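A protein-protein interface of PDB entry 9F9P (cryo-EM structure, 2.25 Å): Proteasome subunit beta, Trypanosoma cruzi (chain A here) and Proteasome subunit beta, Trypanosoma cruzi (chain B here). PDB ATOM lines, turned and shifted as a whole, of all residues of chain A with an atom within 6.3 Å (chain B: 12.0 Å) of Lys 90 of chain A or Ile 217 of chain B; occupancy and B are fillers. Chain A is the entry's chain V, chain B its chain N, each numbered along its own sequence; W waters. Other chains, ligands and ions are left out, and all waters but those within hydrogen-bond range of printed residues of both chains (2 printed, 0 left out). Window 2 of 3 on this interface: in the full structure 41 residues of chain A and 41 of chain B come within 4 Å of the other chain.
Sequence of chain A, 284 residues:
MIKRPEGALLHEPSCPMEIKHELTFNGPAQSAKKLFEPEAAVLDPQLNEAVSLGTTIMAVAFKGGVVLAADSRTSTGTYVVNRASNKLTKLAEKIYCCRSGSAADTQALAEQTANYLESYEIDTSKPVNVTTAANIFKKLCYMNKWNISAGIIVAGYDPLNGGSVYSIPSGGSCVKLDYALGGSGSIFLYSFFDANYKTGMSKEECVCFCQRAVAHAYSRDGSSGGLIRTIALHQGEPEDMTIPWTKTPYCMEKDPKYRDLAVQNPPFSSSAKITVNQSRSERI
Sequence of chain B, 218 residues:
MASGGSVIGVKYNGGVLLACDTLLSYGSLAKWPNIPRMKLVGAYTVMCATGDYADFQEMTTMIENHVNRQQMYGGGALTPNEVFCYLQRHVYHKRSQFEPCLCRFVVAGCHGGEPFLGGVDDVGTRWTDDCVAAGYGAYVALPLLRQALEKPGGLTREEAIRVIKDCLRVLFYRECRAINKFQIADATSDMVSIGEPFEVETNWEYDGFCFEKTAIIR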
ATOM      1  N   LEU A  88      19.682 -19.848   4.344  1.00  0.00           N
ATOM      2  CA  LEU A  88      20.015 -20.453   5.622  1.00  0.00           C
ATOM      3  C   LEU A  88      18.797 -21.158   6.214  1.00  0.00           C
ATOM      4  O   LEU A  88      17.910 -20.525   6.740  1.00  0.00           O
ATOM      5  CB  LEU A  88      20.535 -19.363   6.560  1.00  0.00           C
ATOM      6  CG  LEU A  88      21.581 -18.437   5.941  1.00  0.00           C
ATOM      7  CD1 LEU A  88      22.051 -17.405   6.928  1.00  0.00           C
ATOM      8  CD2 LEU A  88      22.772 -19.219   5.474  1.00  0.00           C
ATOM      9  N   THR A  89      18.789 -22.473   6.161  1.00  0.00           N
ATOM     10  CA  THR A  89      17.652 -23.304   6.511  1.00  0.00           C
ATOM     11  C   THR A  89      17.885 -24.022   7.834  1.00  0.00           C
ATOM     12  O   THR A  89      18.923 -24.634   8.032  1.00  0.00           O
ATOM     13  CB  THR A  89      17.423 -24.268   5.349  1.00  0.00           C
ATOM     14  OG1 THR A  89      17.072 -23.440   4.228  1.00  0.00           O
ATOM     15  CG2 THR A  89      16.312 -25.251   5.638  1.00  0.00           C
ATOM     16  N   LYS A  90      16.909 -23.983   8.728  1.00  0.00           N
ATOM     17  CA  LYS A  90      17.044 -24.575  10.059  1.00  0.00           C
ATOM     18  C   LYS A  90      16.819 -26.092  10.062  1.00  0.00           C
ATOM     19  O   LYS A  90      15.842 -26.539   9.500  1.00  0.00           O
ATOM     20  CB  LYS A  90      16.018 -23.928  10.970  1.00  0.00           C
ATOM     21  CG  LYS A  90      15.903 -24.548  12.339  1.00  0.00           C
ATOM     22  CD  LYS A  90      14.974 -23.757  13.202  1.00  0.00           C
ATOM     23  CE  LYS A  90      14.370 -24.628  14.282  1.00  0.00           C
ATOM     24  NZ  LYS A  90      13.961 -23.822  15.468  1.00  0.00           N
ATOM     25  N   LEU A  91      17.743 -26.871  10.648  1.00  0.00           N
ATOM     26  CA  LEU A  91      17.616 -28.319  10.759  1.00  0.00           C
ATOM     27  C   LEU A  91      17.295 -28.774  12.195  1.00  0.00           C
ATOM     28  O   LEU A  91      16.716 -29.819  12.385  1.00  0.00           O
ATOM     29  CB  LEU A  91      18.888 -29.001  10.293  1.00  0.00           C
ATOM     30  CG  LEU A  91      19.306 -28.823   8.842  1.00  0.00           C
ATOM     31  CD1 LEU A  91      20.673 -29.477   8.617  1.00  0.00           C
ATOM     32  CD2 LEU A  91      18.310 -29.420   7.865  1.00  0.00           C
ATOM     33  N   ALA A  92      17.653 -28.000  13.202  1.00  0.00           N
ATOM     34  CA  ALA A  92      17.374 -28.260  14.609  1.00  0.00           C
ATOM     35  C   ALA A  92      17.649 -26.966  15.337  1.00  0.00           C
ATOM     36  O   ALA A  92      18.040 -26.000  14.704  1.00  0.00           O
ATOM     37  CB  ALA A  92      18.261 -29.355  15.147  1.00  0.00           C
ATOM     38  N   GLU A  93      17.445 -26.882  16.636  1.00  0.00           N
ATOM     39  CA  GLU A  93      17.512 -25.571  17.257  1.00  0.00           C
ATOM     40  C   GLU A  93      18.870 -24.896  16.979  1.00  0.00           C
ATOM     41  O   GLU A  93      18.895 -23.700  16.668  1.00  0.00           O
ATOM     42  CB  GLU A  93      17.208 -25.667  18.754  1.00  0.00           C
ATOM     43  CG  GLU A  93      17.383 -24.324  19.483  1.00  0.00           C
ATOM     44  CD  GLU A  93      16.870 -24.198  20.921  1.00  0.00           C
ATOM     45  OE1 GLU A  93      17.146 -25.105  21.755  1.00  0.00           O
ATOM     46  OE2 GLU A  93      16.226 -23.155  21.227  1.00  0.00           O
ATOM     47  N   ILE A  95      21.415 -26.116  14.759  1.00  0.00           N
ATOM     48  CA  ILE A  95      22.057 -26.628  13.577  1.00  0.00           C
ATOM     49  C   ILE A  95      21.338 -26.131  12.329  1.00  0.00           C
ATOM     50  O   ILE A  95      20.165 -26.411  12.151  1.00  0.00           O
ATOM     51  CB  ILE A  95      22.033 -28.155  13.608  1.00  0.00           C
ATOM     52  CG1 ILE A  95      22.585 -28.743  14.913  1.00  0.00           C
ATOM     53  CG2 ILE A  95      22.770 -28.729  12.411  1.00  0.00           C
ATOM     54  CD1 ILE A  95      22.330 -30.241  14.964  1.00  0.00           C
ATOM     55  N   TYR A  96      22.092 -25.484  11.426  1.00  0.00           N
ATOM     56  CA  TYR A  96      21.576 -24.959  10.179  1.00  0.00           C
ATOM     57  C   TYR A  96      22.350 -25.486   9.003  1.00  0.00           C
ATOM     58  O   TYR A  96      23.480 -25.857   9.157  1.00  0.00           O
ATOM     59  CB  TYR A  96      21.673 -23.449  10.117  1.00  0.00           C
ATOM     60  CG  TYR A  96      20.571 -22.745  10.833  1.00  0.00           C
ATOM     61  CD1 TYR A  96      20.417 -22.866  12.206  1.00  0.00           C
ATOM     62  CD2 TYR A  96      19.651 -21.981  10.146  1.00  0.00           C
ATOM     63  CE1 TYR A  96      19.367 -22.260  12.870  1.00  0.00           C
ATOM     64  CE2 TYR A  96      18.619 -21.323  10.810  1.00  0.00           C
ATOM     65  CZ  TYR A  96      18.484 -21.470  12.176  1.00  0.00           C
ATOM     66  OH  TYR A  96      17.472 -20.818  12.822  1.00  0.00           O
ATOM     67  N   CYS A  97      21.733 -25.476   7.831  1.00  0.00           N
ATOM     68  CA  CYS A  97      22.483 -25.641   6.603  1.00  0.00           C
ATOM     69  C   CYS A  97      22.431 -24.403   5.682  1.00  0.00           C
ATOM     70  O   CYS A  97      21.628 -23.506   5.880  1.00  0.00           O
ATOM     71  CB  CYS A  97      22.015 -26.875   5.888  1.00  0.00           C
ATOM     72  SG  CYS A  97      20.349 -26.727   5.222  1.00  0.00           S
ATOM     73  N   GLN A 107      15.617 -27.862  -1.177  1.00  0.00           N
ATOM     74  CA  GLN A 107      14.505 -27.708  -0.257  1.00  0.00           C
ATOM     75  C   GLN A 107      14.024 -29.101   0.152  1.00  0.00           C
ATOM     76  O   GLN A 107      13.832 -29.369   1.331  1.00  0.00           O
ATOM     77  CB  GLN A 107      13.367 -26.868  -0.817  1.00  0.00           C
ATOM     78  CG  GLN A 107      13.638 -25.362  -0.933  1.00  0.00           C
ATOM     79  CD  GLN A 107      12.440 -24.658  -1.579  1.00  0.00           C
ATOM     80  OE1 GLN A 107      11.313 -25.163  -1.540  1.00  0.00           O
ATOM     81  NE2 GLN A 107      12.648 -23.476  -2.152  1.00  0.00           N
ATOM     82  N   ALA A 110      16.650 -30.852   2.581  1.00  0.00           N
ATOM     83  CA  ALA A 110      16.713 -30.240   3.896  1.00  0.00           C
ATOM     84  C   ALA A 110      15.532 -30.679   4.764  1.00  0.00           C
ATOM     85  O   ALA A 110      15.731 -30.972   5.933  1.00  0.00           O
ATOM     86  CB  ALA A 110      16.767 -28.742   3.808  1.00  0.00           C
ATOM     87  N   GLU A 111      14.324 -30.683   4.178  1.00  0.00           N
ATOM     88  CA  GLU A 111      13.086 -31.040   4.864  1.00  0.00           C
ATOM     89  C   GLU A 111      13.129 -32.483   5.358  1.00  0.00           C
ATOM     90  O   GLU A 111      12.763 -32.744   6.491  1.00  0.00           O
ATOM     91  CB  GLU A 111      11.854 -30.862   3.957  1.00  0.00           C
ATOM     92  CG  GLU A 111      11.327 -29.416   3.886  1.00  0.00           C
ATOM     93  CD  GLU A 111      10.600 -28.956   2.601  1.00  0.00           C
ATOM     94  OE1 GLU A 111       9.875 -29.775   1.971  1.00  0.00           O
ATOM     95  OE2 GLU A 111      10.709 -27.746   2.239  1.00  0.00           O
ATOM     96  N   ALA A 114      15.611 -32.774   8.337  1.00  0.00           N
ATOM     97  CA  ALA A 114      15.017 -32.198   9.533  1.00  0.00           C
ATOM     98  C   ALA A 114      13.986 -33.101  10.201  1.00  0.00           C
ATOM     99  O   ALA A 114      13.863 -33.074  11.422  1.00  0.00           O
ATOM    100  CB  ALA A 114      14.373 -30.856   9.215  1.00  0.00           C
ATOM    101  N   CYS B 210      11.772 -10.151   5.563  1.00  0.00           N
ATOM    102  CA  CYS B 210      12.463 -10.468   6.804  1.00  0.00           C
ATOM    103  C   CYS B 210      12.774 -11.966   6.952  1.00  0.00           C
ATOM    104  O   CYS B 210      12.147 -12.818   6.317  1.00  0.00           O
ATOM    105  CB  CYS B 210      11.635  -9.987   7.990  1.00  0.00           C
ATOM    106  SG  CYS B 210      10.459 -11.231   8.586  1.00  0.00           S
ATOM    107  N   PHE B 211      13.744 -12.265   7.835  1.00  0.00           N
ATOM    108  CA  PHE B 211      14.353 -13.590   7.978  1.00  0.00           C
ATOM    109  C   PHE B 211      13.328 -14.648   8.384  1.00  0.00           C
ATOM    110  O   PHE B 211      13.282 -15.722   7.799  1.00  0.00           O
ATOM    111  CB  PHE B 211      15.516 -13.512   8.976  1.00  0.00           C
ATOM    112  CG  PHE B 211      16.412 -14.707   9.050  1.00  0.00           C
ATOM    113  CD1 PHE B 211      15.992 -15.875   9.674  1.00  0.00           C
ATOM    114  CD2 PHE B 211      17.705 -14.655   8.531  1.00  0.00           C
ATOM    115  CE1 PHE B 211      16.829 -16.991   9.734  1.00  0.00           C
ATOM    116  CE2 PHE B 211      18.546 -15.770   8.606  1.00  0.00           C
ATOM    117  CZ  PHE B 211      18.102 -16.939   9.201  1.00  0.00           C
ATOM    118  N   GLU B 212      12.422 -14.302   9.303  1.00  0.00           N
ATOM    119  CA  GLU B 212      11.406 -15.242   9.765  1.00  0.00           C
ATOM    120  C   GLU B 212      10.408 -15.608   8.647  1.00  0.00           C
ATOM    121  O   GLU B 212      10.136 -16.787   8.438  1.00  0.00           O
ATOM    122  CB  GLU B 212      10.743 -14.679  11.019  1.00  0.00           C
ATOM    123  CG  GLU B 212       9.619 -15.563  11.550  1.00  0.00           C
ATOM    124  CD  GLU B 212       8.292 -14.851  11.818  1.00  0.00           C
ATOM    125  OE1 GLU B 212       8.251 -13.989  12.735  1.00  0.00           O
ATOM    126  OE2 GLU B 212       7.300 -15.144  11.094  1.00  0.00           O
ATOM    127  N   LYS B 213       9.878 -14.634   7.900  1.00  0.00           N
ATOM    128  CA  LYS B 213       8.852 -14.910   6.898  1.00  0.00           C
ATOM    129  C   LYS B 213       9.365 -15.672   5.674  1.00  0.00           C
ATOM    130  O   LYS B 213       8.617 -16.439   5.093  1.00  0.00           O
ATOM    131  CB  LYS B 213       8.272 -13.623   6.314  1.00  0.00           C
ATOM    132  CG  LYS B 213       7.418 -12.793   7.241  1.00  0.00           C
ATOM    133  CD  LYS B 213       5.957 -12.812   6.885  1.00  0.00           C
ATOM    134  CE  LYS B 213       5.230 -11.664   7.548  1.00  0.00           C
ATOM    135  NZ  LYS B 213       3.831 -12.035   7.832  1.00  0.00           N
ATOM    136  N   THR B 214      10.615 -15.452   5.278  1.00  0.00           N
ATOM    137  CA  THR B 214      11.203 -16.090   4.106  1.00  0.00           C
ATOM    138  C   THR B 214      11.791 -17.479   4.416  1.00  0.00           C
ATOM    139  O   THR B 214      12.196 -18.196   3.494  1.00  0.00           O
ATOM    140  CB  THR B 214      12.262 -15.158   3.483  1.00  0.00           C
ATOM    141  OG1 THR B 214      13.265 -14.818   4.452  1.00  0.00           O
ATOM    142  CG2 THR B 214      11.664 -13.864   2.956  1.00  0.00           C
ATOM    143  N   ALA B 215      11.839 -17.879   5.694  1.00  0.00           N
ATOM    144  CA  ALA B 215      12.359 -19.187   6.089  1.00  0.00           C
ATOM    145  C   ALA B 215      11.571 -20.349   5.483  1.00  0.00           C
ATOM    146  O   ALA B 215      10.355 -20.328   5.435  1.00  0.00           O
ATOM    147  CB  ALA B 215      12.394 -19.302   7.596  1.00  0.00           C
ATOM    148  N   ILE B 216      12.287 -21.390   5.044  1.00  0.00           N
ATOM    149  CA  ILE B 216      11.675 -22.562   4.419  1.00  0.00           C
ATOM    150  C   ILE B 216      11.116 -23.531   5.464  1.00  0.00           C
ATOM    151  O   ILE B 216      10.111 -24.157   5.196  1.00  0.00           O
ATOM    152  CB  ILE B 216      12.697 -23.280   3.504  1.00  0.00           C
ATOM    153  CG1 ILE B 216      13.297 -22.357   2.429  1.00  0.00           C
ATOM    154  CG2 ILE B 216      12.078 -24.513   2.882  1.00  0.00           C
ATOM    155  CD1 ILE B 216      12.289 -21.812   1.446  1.00  0.00           C
ATOM    156  N   ILE B 217      11.809 -23.693   6.599  1.00  0.00           N
ATOM    157  CA  ILE B 217      11.405 -24.552   7.705  1.00  0.00           C
ATOM    158  C   ILE B 217      11.228 -23.712   8.988  1.00  0.00           C
ATOM    159  O   ILE B 217      12.139 -22.988   9.409  1.00  0.00           O
ATOM    160  CB  ILE B 217      12.447 -25.673   7.903  1.00  0.00           C
ATOM    161  CG1 ILE B 217      12.558 -26.621   6.708  1.00  0.00           C
ATOM    162  CG2 ILE B 217      12.195 -26.460   9.180  1.00  0.00           C
ATOM    163  CD1 ILE B 217      13.835 -27.476   6.741  1.00  0.00           C
ATOM    164  N   ARG B 218      10.064 -23.890   9.643  1.00  0.00           N
ATOM    165  CA  ARG B 218       9.547 -22.975  10.656  1.00  0.00           C
ATOM    166  C   ARG B 218       9.832 -23.523  12.062  1.00  0.00           C
ATOM    167  O   ARG B 218       9.273 -22.935  13.015  1.00  0.00           O
ATOM    168  CB  ARG B 218       8.030 -22.777  10.520  1.00  0.00           C
ATOM    169  CG  ARG B 218       7.500 -22.668   9.091  1.00  0.00           C
ATOM    170  CD  ARG B 218       7.224 -21.247   8.614  1.00  0.00           C
ATOM    171  NE  ARG B 218       6.043 -21.151   7.751  1.00  0.00           N
ATOM    172  CZ  ARG B 218       4.785 -21.375   8.140  1.00  0.00           C
ATOM    173  NH1 ARG B 218       3.791 -21.215   7.287  1.00  0.00           N
ATOM    174  NH2 ARG B 218       4.517 -21.746   9.382  1.00  0.00           N
ATOM    175  OXT ARG B 218      10.602 -24.513  12.160  1.00  0.00           O
HETATM  176  O   HOH W   1      14.453 -22.320   8.010  1.00  0.00           O
HETATM  177  O   HOH W   2      15.565 -20.702   4.660  1.00  0.00           O
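Of chain B, only Ile 217 (3.5 Å) comes within 4 Å of Lys 90 of chain A. Ile 217 of chain B touches just these residues of chain A: Thr 89 and Lys 90. Of chain B, only Ile 217 (3.5 Å) comes within 4 Å of Thr 89 of chain A. No residue of chain B comes within 4 Å of Leu 91 of chain A. No residue of chain B comes within 4 Å of Tyr 96 of chain A. No residue of chain B comes within 4 Å of Cys 97 of chain A. No residue of chain B comes within 4 Å of Ala 110 of chain A. No residue of chain B comes within 4 Å of Ala 114 of chain A. Of the printed residues of chain A, Ile 216 of chain B touches Gln 107 and Glu 111. Printed residues of chain B within 4 Å of Gln 107 of chain A: Ile 216 (3.98 Å). Arg 218 of chain B touches none of the printed residues of chain A. The nearest residue of chain B that does not touch Lys 90 of chain A is Arg 218 of chain B (4.3 Å).
Water W1 bridges the backbone carbonyl oxygen (O) of Ile 217 of chain B and the backbone NH (N) of Lys 90 of chain A. Water W2 lies within hydrogen-bond range of O of Leu 88 of chain A (3.1 Å), OG1 of Thr 89 of chain A (3.2 Å) and N of Ile 216 of chain B (3.4 Å).
CG2 of Thr 89 of chain A touches CD1 of Ile 217 of chain B (3.5 Å). Ile 217 of chain B touches Lys 90 of chain A. Gln 107 of chain A touches Ile 216 of chain B (NE2 to CD1, 3.98 Å). Ile 216 of chain B touches Glu 111 of chain A (CG2 to OE2, 3.6 Å).
Of the 13 printed residues of chain A, 4 touch a printed residue of chain B. Among the printed residues, no Asp or Glu carboxylate lies within 4 Å of a Lys or Arg side-chain nitrogen of the other chain.
The backbone carbonyl oxygen (O) of Thr 89 of chain A is in hydrogen-bond range of the backbone NH (N) of Cys 97 of chain A (2.9 Å).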
